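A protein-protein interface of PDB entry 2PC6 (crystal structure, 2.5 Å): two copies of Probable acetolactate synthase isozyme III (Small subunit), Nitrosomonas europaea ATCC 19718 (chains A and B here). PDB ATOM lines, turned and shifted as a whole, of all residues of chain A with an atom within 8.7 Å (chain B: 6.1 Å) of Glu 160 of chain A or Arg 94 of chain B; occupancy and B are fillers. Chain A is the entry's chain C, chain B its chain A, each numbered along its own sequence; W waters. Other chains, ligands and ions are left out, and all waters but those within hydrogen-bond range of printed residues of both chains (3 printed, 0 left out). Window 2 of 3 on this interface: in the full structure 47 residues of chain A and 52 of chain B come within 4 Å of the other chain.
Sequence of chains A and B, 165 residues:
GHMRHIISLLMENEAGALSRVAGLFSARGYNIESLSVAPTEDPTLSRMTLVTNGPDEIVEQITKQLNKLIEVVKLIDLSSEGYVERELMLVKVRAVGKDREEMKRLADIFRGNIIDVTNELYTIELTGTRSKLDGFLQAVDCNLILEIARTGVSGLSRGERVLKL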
ATOM      1  N   GLY A  82     -17.050  26.826   7.465  1.00  0.00           N
ATOM      2  CA  GLY A  82     -18.308  26.659   8.249  1.00  0.00           C
ATOM      3  C   GLY A  82     -18.809  25.198   8.246  1.00  0.00           C
ATOM      4  O   GLY A  82     -18.796  24.543   7.191  1.00  0.00           O
ATOM      5  N   SER A 157     -19.731  20.037   5.898  1.00  0.00           N
ATOM      6  CA  SER A 157     -19.600  21.453   5.673  1.00  0.00           C
ATOM      7  C   SER A 157     -20.984  22.105   5.726  1.00  0.00           C
ATOM      8  O   SER A 157     -22.012  21.467   5.473  1.00  0.00           O
ATOM      9  CB  SER A 157     -18.932  21.692   4.331  1.00  0.00           C
ATOM     10  OG  SER A 157     -17.723  20.938   4.243  1.00  0.00           O
ATOM     11  N   ARG A 158     -21.010  23.379   6.078  1.00  0.00           N
ATOM     12  CA  ARG A 158     -22.246  24.152   5.957  1.00  0.00           C
ATOM     13  C   ARG A 158     -22.540  24.475   4.499  1.00  0.00           C
ATOM     14  O   ARG A 158     -21.612  24.609   3.682  1.00  0.00           O
ATOM     15  CB  ARG A 158     -22.172  25.442   6.782  1.00  0.00           C
ATOM     16  CG  ARG A 158     -22.781  25.252   8.155  1.00  0.00           C
ATOM     17  CD  ARG A 158     -23.360  26.535   8.740  1.00  0.00           C
ATOM     18  NE  ARG A 158     -23.417  26.401  10.201  1.00  0.00           N
ATOM     19  CZ  ARG A 158     -24.434  25.891  10.914  1.00  0.00           C
ATOM     20  NH1 ARG A 158     -25.558  25.462  10.326  1.00  0.00           N
ATOM     21  NH2 ARG A 158     -24.326  25.826  12.244  1.00  0.00           N
ATOM     22  N   GLY A 159     -23.824  24.624   4.180  1.00  0.00           N
ATOM     23  CA  GLY A 159     -24.259  25.063   2.845  1.00  0.00           C
ATOM     24  C   GLY A 159     -23.908  24.113   1.713  1.00  0.00           C
ATOM     25  O   GLY A 159     -23.877  22.892   1.888  1.00  0.00           O
ATOM     26  N   GLU A 160     -23.592  24.682   0.560  1.00  0.00           N
ATOM     27  CA  GLU A 160     -23.435  23.923  -0.675  1.00  0.00           C
ATOM     28  C   GLU A 160     -22.119  23.162  -0.763  1.00  0.00           C
ATOM     29  O   GLU A 160     -21.994  22.233  -1.568  1.00  0.00           O
ATOM     30  CB  GLU A 160     -23.582  24.851  -1.889  1.00  0.00           C
ATOM     31  CG  GLU A 160     -24.955  25.441  -2.022  1.00  0.00           C
ATOM     32  CD  GLU A 160     -25.955  24.500  -2.698  1.00  0.00           C
ATOM     33  OE1 GLU A 160     -25.562  23.453  -3.250  1.00  0.00           O
ATOM     34  OE2 GLU A 160     -27.156  24.811  -2.689  1.00  0.00           O
ATOM     35  N   ARG A 161     -21.132  23.566   0.025  1.00  0.00           N
ATOM     36  CA  ARG A 161     -19.891  22.794   0.116  1.00  0.00           C
ATOM     37  C   ARG A 161     -20.158  21.298   0.426  1.00  0.00           C
ATOM     38  O   ARG A 161     -20.769  20.971   1.431  1.00  0.00           O
ATOM     39  CB  ARG A 161     -19.008  23.395   1.196  1.00  0.00           C
ATOM     40  CG  ARG A 161     -17.595  22.882   1.205  1.00  0.00           C
ATOM     41  CD  ARG A 161     -16.746  23.777   2.122  1.00  0.00           C
ATOM     42  NE  ARG A 161     -16.755  25.155   1.638  1.00  0.00           N
ATOM     43  CZ  ARG A 161     -15.981  25.579   0.646  1.00  0.00           C
ATOM     44  NH1 ARG A 161     -15.142  24.722   0.073  1.00  0.00           N
ATOM     45  NH2 ARG A 161     -16.030  26.840   0.225  1.00  0.00           N
ATOM     46  N   VAL A 162     -19.720  20.415  -0.463  1.00  0.00           N
ATOM     47  CA  VAL A 162     -19.819  18.976  -0.264  1.00  0.00           C
ATOM     48  C   VAL A 162     -18.522  18.263  -0.655  1.00  0.00           C
ATOM     49  O   VAL A 162     -17.834  18.659  -1.587  1.00  0.00           O
ATOM     50  CB  VAL A 162     -21.004  18.363  -1.053  1.00  0.00           C
ATOM     51  CG1 VAL A 162     -22.268  19.090  -0.744  1.00  0.00           C
ATOM     52  CG2 VAL A 162     -20.748  18.392  -2.560  1.00  0.00           C
ATOM     53  N   LEU A 163     -18.201  17.188   0.047  1.00  0.00           N
ATOM     54  CA  LEU A 163     -16.910  16.533  -0.117  1.00  0.00           C
ATOM     55  C   LEU A 163     -16.724  15.760  -1.433  1.00  0.00           C
ATOM     56  O   LEU A 163     -15.699  15.907  -2.112  1.00  0.00           O
ATOM     57  CB  LEU A 163     -16.686  15.644   1.080  1.00  0.00           C
ATOM     58  CG  LEU A 163     -15.268  15.178   1.350  1.00  0.00           C
ATOM     59  CD1 LEU A 163     -14.408  16.368   1.705  1.00  0.00           C
ATOM     60  CD2 LEU A 163     -15.327  14.177   2.494  1.00  0.00           C
ATOM     61  N   LYS A 164     -17.703  14.949  -1.828  1.00  0.00           N
ATOM     62  CA  LYS A 164     -17.578  14.253  -3.114  1.00  0.00           C
ATOM     63  C   LYS A 164     -17.392  15.211  -4.290  1.00  0.00           C
ATOM     64  O   LYS A 164     -16.887  14.785  -5.336  1.00  0.00           O
ATOM     65  CB  LYS A 164     -18.691  13.206  -3.363  1.00  0.00           C
ATOM     66  CG  LYS A 164     -20.138  13.705  -3.439  1.00  0.00           C
ATOM     67  CD  LYS A 164     -21.034  12.587  -3.934  1.00  0.00           C
ATOM     68  CE  LYS A 164     -22.494  12.852  -3.606  1.00  0.00           C
ATOM     69  NZ  LYS A 164     -23.407  11.786  -4.162  1.00  0.00           N
ATOM     70  N   LEU A 165     -17.748  16.494  -4.097  1.00  0.00           N
ATOM     71  CA  LEU A 165     -17.349  17.600  -5.028  1.00  0.00           C
ATOM     72  C   LEU A 165     -16.116  18.450  -4.603  1.00  0.00           C
ATOM     73  O   LEU A 165     -15.432  19.056  -5.456  1.00  0.00           O
ATOM     74  CB  LEU A 165     -18.531  18.526  -5.398  1.00  0.00           C
ATOM     75  OXT LEU A 165     -15.746  18.577  -3.431  1.00  0.00           O
ATOM     76  N   LYS B  92     -27.534  15.740   3.935  1.00  0.00           N
ATOM     77  CA  LYS B  92     -27.729  17.044   3.282  1.00  0.00           C
ATOM     78  C   LYS B  92     -28.480  16.828   1.979  1.00  0.00           C
ATOM     79  O   LYS B  92     -28.044  16.048   1.154  1.00  0.00           O
ATOM     80  CB  LYS B  92     -26.387  17.756   3.064  1.00  0.00           C
ATOM     81  CG  LYS B  92     -26.444  18.968   2.175  1.00  0.00           C
ATOM     82  CD  LYS B  92     -25.029  19.528   1.868  1.00  0.00           C
ATOM     83  CE  LYS B  92     -24.334  19.918   3.171  1.00  0.00           C
ATOM     84  NZ  LYS B  92     -22.928  20.344   2.957  1.00  0.00           N
ATOM     85  N   VAL B  93     -29.607  17.515   1.816  1.00  0.00           N
ATOM     86  CA  VAL B  93     -30.539  17.266   0.738  1.00  0.00           C
ATOM     87  C   VAL B  93     -30.839  18.550   0.007  1.00  0.00           C
ATOM     88  O   VAL B  93     -30.902  19.627   0.606  1.00  0.00           O
ATOM     89  CB  VAL B  93     -31.919  16.703   1.245  1.00  0.00           C
ATOM     90  CG1 VAL B  93     -31.789  15.290   1.740  1.00  0.00           C
ATOM     91  CG2 VAL B  93     -32.543  17.640   2.345  1.00  0.00           C
ATOM     92  N   ARG B  94     -31.015  18.411  -1.297  1.00  0.00           N
ATOM     93  CA  ARG B  94     -31.412  19.456  -2.172  1.00  0.00           C
ATOM     94  C   ARG B  94     -32.884  19.678  -1.876  1.00  0.00           C
ATOM     95  O   ARG B  94     -33.659  18.727  -1.829  1.00  0.00           O
ATOM     96  CB  ARG B  94     -31.183  18.955  -3.607  1.00  0.00           C
ATOM     97  CG  ARG B  94     -31.759  19.788  -4.764  1.00  0.00           C
ATOM     98  CD  ARG B  94     -31.196  21.206  -4.843  1.00  0.00           C
ATOM     99  NE  ARG B  94     -29.762  21.325  -5.086  1.00  0.00           N
ATOM    100  CZ  ARG B  94     -28.931  22.002  -4.301  1.00  0.00           C
ATOM    101  NH1 ARG B  94     -29.396  22.576  -3.196  1.00  0.00           N
ATOM    102  NH2 ARG B  94     -27.640  22.095  -4.592  1.00  0.00           N
ATOM    103  N   ALA B  95     -33.280  20.921  -1.643  1.00  0.00           N
ATOM    104  CA  ALA B  95     -34.644  21.170  -1.265  1.00  0.00           C
ATOM    105  C   ALA B  95     -35.109  22.474  -1.872  1.00  0.00           C
ATOM    106  O   ALA B  95     -34.941  23.522  -1.266  1.00  0.00           O
ATOM    107  CB  ALA B  95     -34.817  21.156   0.293  1.00  0.00           C
ATOM    108  N   VAL B  96     -35.699  22.378  -3.062  1.00  0.00           N
ATOM    109  CA  VAL B  96     -36.248  23.518  -3.775  1.00  0.00           C
ATOM    110  C   VAL B  96     -37.694  23.239  -4.236  1.00  0.00           C
ATOM    111  O   VAL B  96     -38.052  22.087  -4.553  1.00  0.00           O
ATOM    112  CB  VAL B  96     -35.314  23.976  -4.966  1.00  0.00           C
ATOM    113  CG1 VAL B  96     -33.846  23.567  -4.723  1.00  0.00           C
ATOM    114  CG2 VAL B  96     -35.784  23.434  -6.314  1.00  0.00           C
ATOM    115  N   ASP B  99     -40.248  20.368  -3.025  1.00  0.00           N
ATOM    116  CA  ASP B  99     -39.447  19.397  -2.294  1.00  0.00           C
ATOM    117  C   ASP B  99     -39.049  19.917  -0.939  1.00  0.00           C
ATOM    118  O   ASP B  99     -38.692  19.139  -0.060  1.00  0.00           O
ATOM    119  CB  ASP B  99     -38.229  18.977  -3.086  1.00  0.00           C
ATOM    120  CG  ASP B  99     -38.558  17.933  -4.099  1.00  0.00           C
ATOM    121  OD1 ASP B  99     -39.562  17.226  -3.878  1.00  0.00           O
ATOM    122  OD2 ASP B  99     -37.820  17.813  -5.106  1.00  0.00           O
ATOM    123  N   MET B 103     -39.377  17.343   2.091  1.00  0.00           N
ATOM    124  CA  MET B 103     -38.224  17.116   2.969  1.00  0.00           C
ATOM    125  C   MET B 103     -38.542  17.508   4.376  1.00  0.00           C
ATOM    126  O   MET B 103     -38.123  16.826   5.301  1.00  0.00           O
ATOM    127  CB  MET B 103     -36.987  17.892   2.518  1.00  0.00           C
ATOM    128  CG  MET B 103     -36.369  17.426   1.233  1.00  0.00           C
ATOM    129  SD  MET B 103     -35.810  15.545   1.264  1.00  0.00           S
ATOM    130  CE  MET B 103     -37.470  14.664   0.661  1.00  0.00           C
ATOM    131  N   THR B 118     -30.454  26.604   3.833  1.00  0.00           N
ATOM    132  CA  THR B 118     -30.473  27.706   2.842  1.00  0.00           C
ATOM    133  C   THR B 118     -31.753  27.624   2.005  1.00  0.00           C
ATOM    134  O   THR B 118     -32.553  26.647   2.113  1.00  0.00           O
ATOM    135  CB  THR B 118     -29.360  27.601   1.809  1.00  0.00           C
ATOM    136  OG1 THR B 118     -29.766  26.640   0.824  1.00  0.00           O
ATOM    137  CG2 THR B 118     -28.053  27.197   2.443  1.00  0.00           C
ATOM    138  N   GLU B 120     -32.060  26.572  -0.844  1.00  0.00           N
ATOM    139  CA  GLU B 120     -32.062  25.449  -1.766  1.00  0.00           C
ATOM    140  C   GLU B 120     -31.655  24.154  -1.100  1.00  0.00           C
ATOM    141  O   GLU B 120     -31.658  23.098  -1.732  1.00  0.00           O
ATOM    142  CB  GLU B 120     -31.104  25.727  -2.916  1.00  0.00           C
ATOM    143  CG  GLU B 120     -31.530  26.861  -3.868  1.00  0.00           C
ATOM    144  CD  GLU B 120     -31.168  28.275  -3.375  1.00  0.00           C
ATOM    145  OE1 GLU B 120     -30.226  28.391  -2.561  1.00  0.00           O
ATOM    146  OE2 GLU B 120     -31.825  29.272  -3.815  1.00  0.00           O
ATOM    147  N   LEU B 121     -31.266  24.213   0.168  1.00  0.00           N
ATOM    148  CA  LEU B 121     -30.915  22.968   0.866  1.00  0.00           C
ATOM    149  C   LEU B 121     -31.299  22.840   2.349  1.00  0.00           C
ATOM    150  O   LEU B 121     -31.585  23.829   3.023  1.00  0.00           O
ATOM    151  CB  LEU B 121     -29.449  22.624   0.619  1.00  0.00           C
ATOM    152  CG  LEU B 121     -28.310  23.256   1.385  1.00  0.00           C
ATOM    153  CD1 LEU B 121     -28.223  22.729   2.847  1.00  0.00           C
ATOM    154  CD2 LEU B 121     -27.011  22.917   0.634  1.00  0.00           C
ATOM    155  N   TYR B 122     -31.317  21.605   2.842  1.00  0.00           N
ATOM    156  CA  TYR B 122     -31.455  21.342   4.263  1.00  0.00           C
ATOM    157  C   TYR B 122     -30.387  20.353   4.674  1.00  0.00           C
ATOM    158  O   TYR B 122     -30.068  19.420   3.897  1.00  0.00           O
ATOM    159  CB  TYR B 122     -32.775  20.663   4.551  1.00  0.00           C
ATOM    160  CG  TYR B 122     -34.046  21.471   4.414  1.00  0.00           C
ATOM    161  CD1 TYR B 122     -34.112  22.801   4.803  1.00  0.00           C
ATOM    162  CD2 TYR B 122     -35.211  20.857   3.969  1.00  0.00           C
ATOM    163  CE1 TYR B 122     -35.286  23.483   4.738  1.00  0.00           C
ATOM    164  CE2 TYR B 122     -36.375  21.527   3.888  1.00  0.00           C
ATOM    165  CZ  TYR B 122     -36.411  22.841   4.267  1.00  0.00           C
ATOM    166  OH  TYR B 122     -37.592  23.509   4.192  1.00  0.00           O
ATOM    167  N   ASN B 143     -31.738  11.037  -5.775  1.00  0.00           N
ATOM    168  CA  ASN B 143     -31.253  12.209  -6.541  1.00  0.00           C
ATOM    169  C   ASN B 143     -31.212  13.501  -5.691  1.00  0.00           C
ATOM    170  O   ASN B 143     -30.400  14.397  -5.933  1.00  0.00           O
ATOM    171  CB  ASN B 143     -32.067  12.403  -7.836  1.00  0.00           C
ATOM    172  CG  ASN B 143     -33.548  12.616  -7.554  1.00  0.00           C
ATOM    173  OD1 ASN B 143     -34.141  11.898  -6.741  1.00  0.00           O
ATOM    174  ND2 ASN B 143     -34.149  13.619  -8.187  1.00  0.00           N
ATOM    175  N   LEU B 144     -32.067  13.555  -4.664  1.00  0.00           N
ATOM    176  CA  LEU B 144     -32.013  14.635  -3.690  1.00  0.00           C
ATOM    177  C   LEU B 144     -30.827  14.552  -2.760  1.00  0.00           C
ATOM    178  O   LEU B 144     -30.421  15.564  -2.208  1.00  0.00           O
ATOM    179  CB  LEU B 144     -33.308  14.785  -2.888  1.00  0.00           C
ATOM    180  CG  LEU B 144     -34.503  14.994  -3.811  1.00  0.00           C
ATOM    181  CD1 LEU B 144     -35.843  15.139  -3.079  1.00  0.00           C
ATOM    182  CD2 LEU B 144     -34.227  16.155  -4.753  1.00  0.00           C
ATOM    183  N   ILE B 145     -30.230  13.400  -2.555  1.00  0.00           N
ATOM    184  CA  ILE B 145     -29.229  13.434  -1.507  1.00  0.00           C
ATOM    185  C   ILE B 145     -27.949  14.089  -1.984  1.00  0.00           C
ATOM    186  O   ILE B 145     -27.368  13.653  -2.963  1.00  0.00           O
ATOM    187  CB  ILE B 145     -28.987  12.067  -0.947  1.00  0.00           C
ATOM    188  CG1 ILE B 145     -30.210  11.694  -0.104  1.00  0.00           C
ATOM    189  CG2 ILE B 145     -27.721  12.058  -0.087  1.00  0.00           C
ATOM    190  CD1 ILE B 145     -30.290  10.226   0.178  1.00  0.00           C
ATOM    191  N   LEU B 146     -27.504  15.152  -1.328  1.00  0.00           N
ATOM    192  CA  LEU B 146     -26.210  15.736  -1.732  1.00  0.00           C
ATOM    193  C   LEU B 146     -24.998  15.022  -1.135  1.00  0.00           C
ATOM    194  O   LEU B 146     -24.011  14.772  -1.840  1.00  0.00           O
ATOM    195  CB  LEU B 146     -26.140  17.226  -1.426  1.00  0.00           C
ATOM    196  CG  LEU B 146     -27.164  18.100  -2.132  1.00  0.00           C
ATOM    197  CD1 LEU B 146     -27.219  19.445  -1.450  1.00  0.00           C
ATOM    198  CD2 LEU B 146     -26.749  18.240  -3.583  1.00  0.00           C
ATOM    199  N   GLU B 147     -25.065  14.725   0.165  1.00  0.00           N
ATOM    200  CA  GLU B 147     -24.066  13.874   0.862  1.00  0.00           C
ATOM    201  C   GLU B 147     -24.657  13.473   2.223  1.00  0.00           C
ATOM    202  O   GLU B 147     -25.668  14.013   2.646  1.00  0.00           O
ATOM    203  CB  GLU B 147     -22.721  14.595   1.041  1.00  0.00           C
ATOM    204  CG  GLU B 147     -22.887  15.867   1.820  1.00  0.00           C
ATOM    205  CD  GLU B 147     -21.616  16.672   1.997  1.00  0.00           C
ATOM    206  OE1 GLU B 147     -20.503  16.180   1.716  1.00  0.00           O
ATOM    207  OE2 GLU B 147     -21.739  17.841   2.428  1.00  0.00           O
HETATM  208  O   HOH W   1     -28.050  27.024  -1.462  1.00  0.00           O
HETATM  209  O   HOH W   2     -19.482  17.984   3.556  1.00  0.00           O
HETATM  210  O   HOH W   3     -19.954  13.515  -0.384  1.00  0.00           O
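The side-chain amino group (NZ) of Lys 92 of chain B sits at hydrogen-bond distance from the backbone carbonyl oxygen (O) of Ser 157 of chain A (2.9 Å).
The side-chain amino group (NZ) of Lys 92 of chain B lies within hydrogen-bond range of the backbone carbonyl oxygen (O) of Gly 159 of chain A, 2.9 Å away.
The side-chain amino group (NZ) of Lys 92 of chain B lies within hydrogen-bond range of the backbone carbonyl oxygen (O) of Arg 161 of chain A, 2.7 Å away.
The guanidinium group (NH2) of Arg 94 of chain B lies within salt-bridge range of the side-chain carboxylate (OE1) of Glu 160 of chain A, 2.8 Å away.
N of Leu 163 of chain A sits at hydrogen-bond distance from OE1 of Glu 147 of chain B (3.0 Å).
The backbone carbonyl oxygen (O) of Arg 161 of chain A lies close to the side-chain carboxylate (OE2) of Glu 147 of chain B (3.4 Å).
O of Lys 92 of chain B is in hydrogen-bond range of N of Leu 146 of chain B.
NZ of Lys 92 of chain B lies within salt-bridge range of OE2 of Glu 147 of chain B, at 2.8 Å.
The backbone carbonyl oxygen (O) of Glu 120 of chain B is in hydrogen-bond range of the guanidinium group (NH1) of Arg 94 of chain B, at 2.7 Å.
The backbone NH (N) of Arg 94 of chain B is in hydrogen-bond range of the backbone carbonyl oxygen (O) of Leu 144 of chain B, 3.0 Å away.
The backbone NH (N) of Leu 121 of chain B lies within hydrogen-bond range of the side-chain hydroxyl (OG1) of Thr 118 of chain B, 2.9 Å away.
Among the printed residues, merely in contact across the chains: Lys 164 of chain A with Leu 146 of chain B (3.0 Å), Gly 159 of chain A with Leu 121 of chain B (3.4 Å), Val 162 of chain A with Glu 147 of chain B (3.4 Å), Val 162 of chain A with Lys 92 of chain B (3.8 Å) and Glu 160 of chain A with Leu 121 of chain B (3.8 Å).
Glu 160 of chain A touches two residues of chain B.
Of the printed residues of chain B, Arg 161 of chain A touches Lys 92 (2.7 Å) and Glu 147 (3.4 Å).
Of the printed residues of chain B, Leu 163 of chain A touches Glu 147.
Of chain A, only Glu 160 (2.8 Å) comes within 4 Å of Arg 94 of chain B.
No residue of chain A comes within 4 Å of Ala 95 of chain B.
The nearest residue of chain B that does not touch Glu 160 of chain A is Glu 120 of chain B (4.1 Å).
The nearest printed residue of chain B that does not touch Leu 163 of chain A is Lys 92 of chain B (6.4 Å).
Hydrophobic or aromatic side chains of chain B that line the printed part of chain A: Leu 121.
Of the 10 printed residues of chain A, 7 touch a printed residue of chain B.
Among the printed residues, Asp or Glu carboxylates within 4 Å of a Lys or Arg side-chain nitrogen of the other chain: Glu 160 of chain A with Arg 94 of chain B (2.8 Å).
No position is printed for both chains.
Of the 11 pairs that touch across the chains among the printed residues, none has its exchanged pair printed and touching as well.
Water W2 bridges OE2 of Glu 147 of chain B and N of Ser 157 of chain A.
Water W1 lies within hydrogen-bond range of OE2 of Glu 160 of chain A, OE1 of Glu 120 of chain B and OG1 of Thr 118 of chain B.
Water W3 lies within hydrogen-bond range of the backbone NH of Lys 164 of chain A (3.0 Å) and the side-chain carboxylate of Glu 147 of chain B (3.4 Å).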
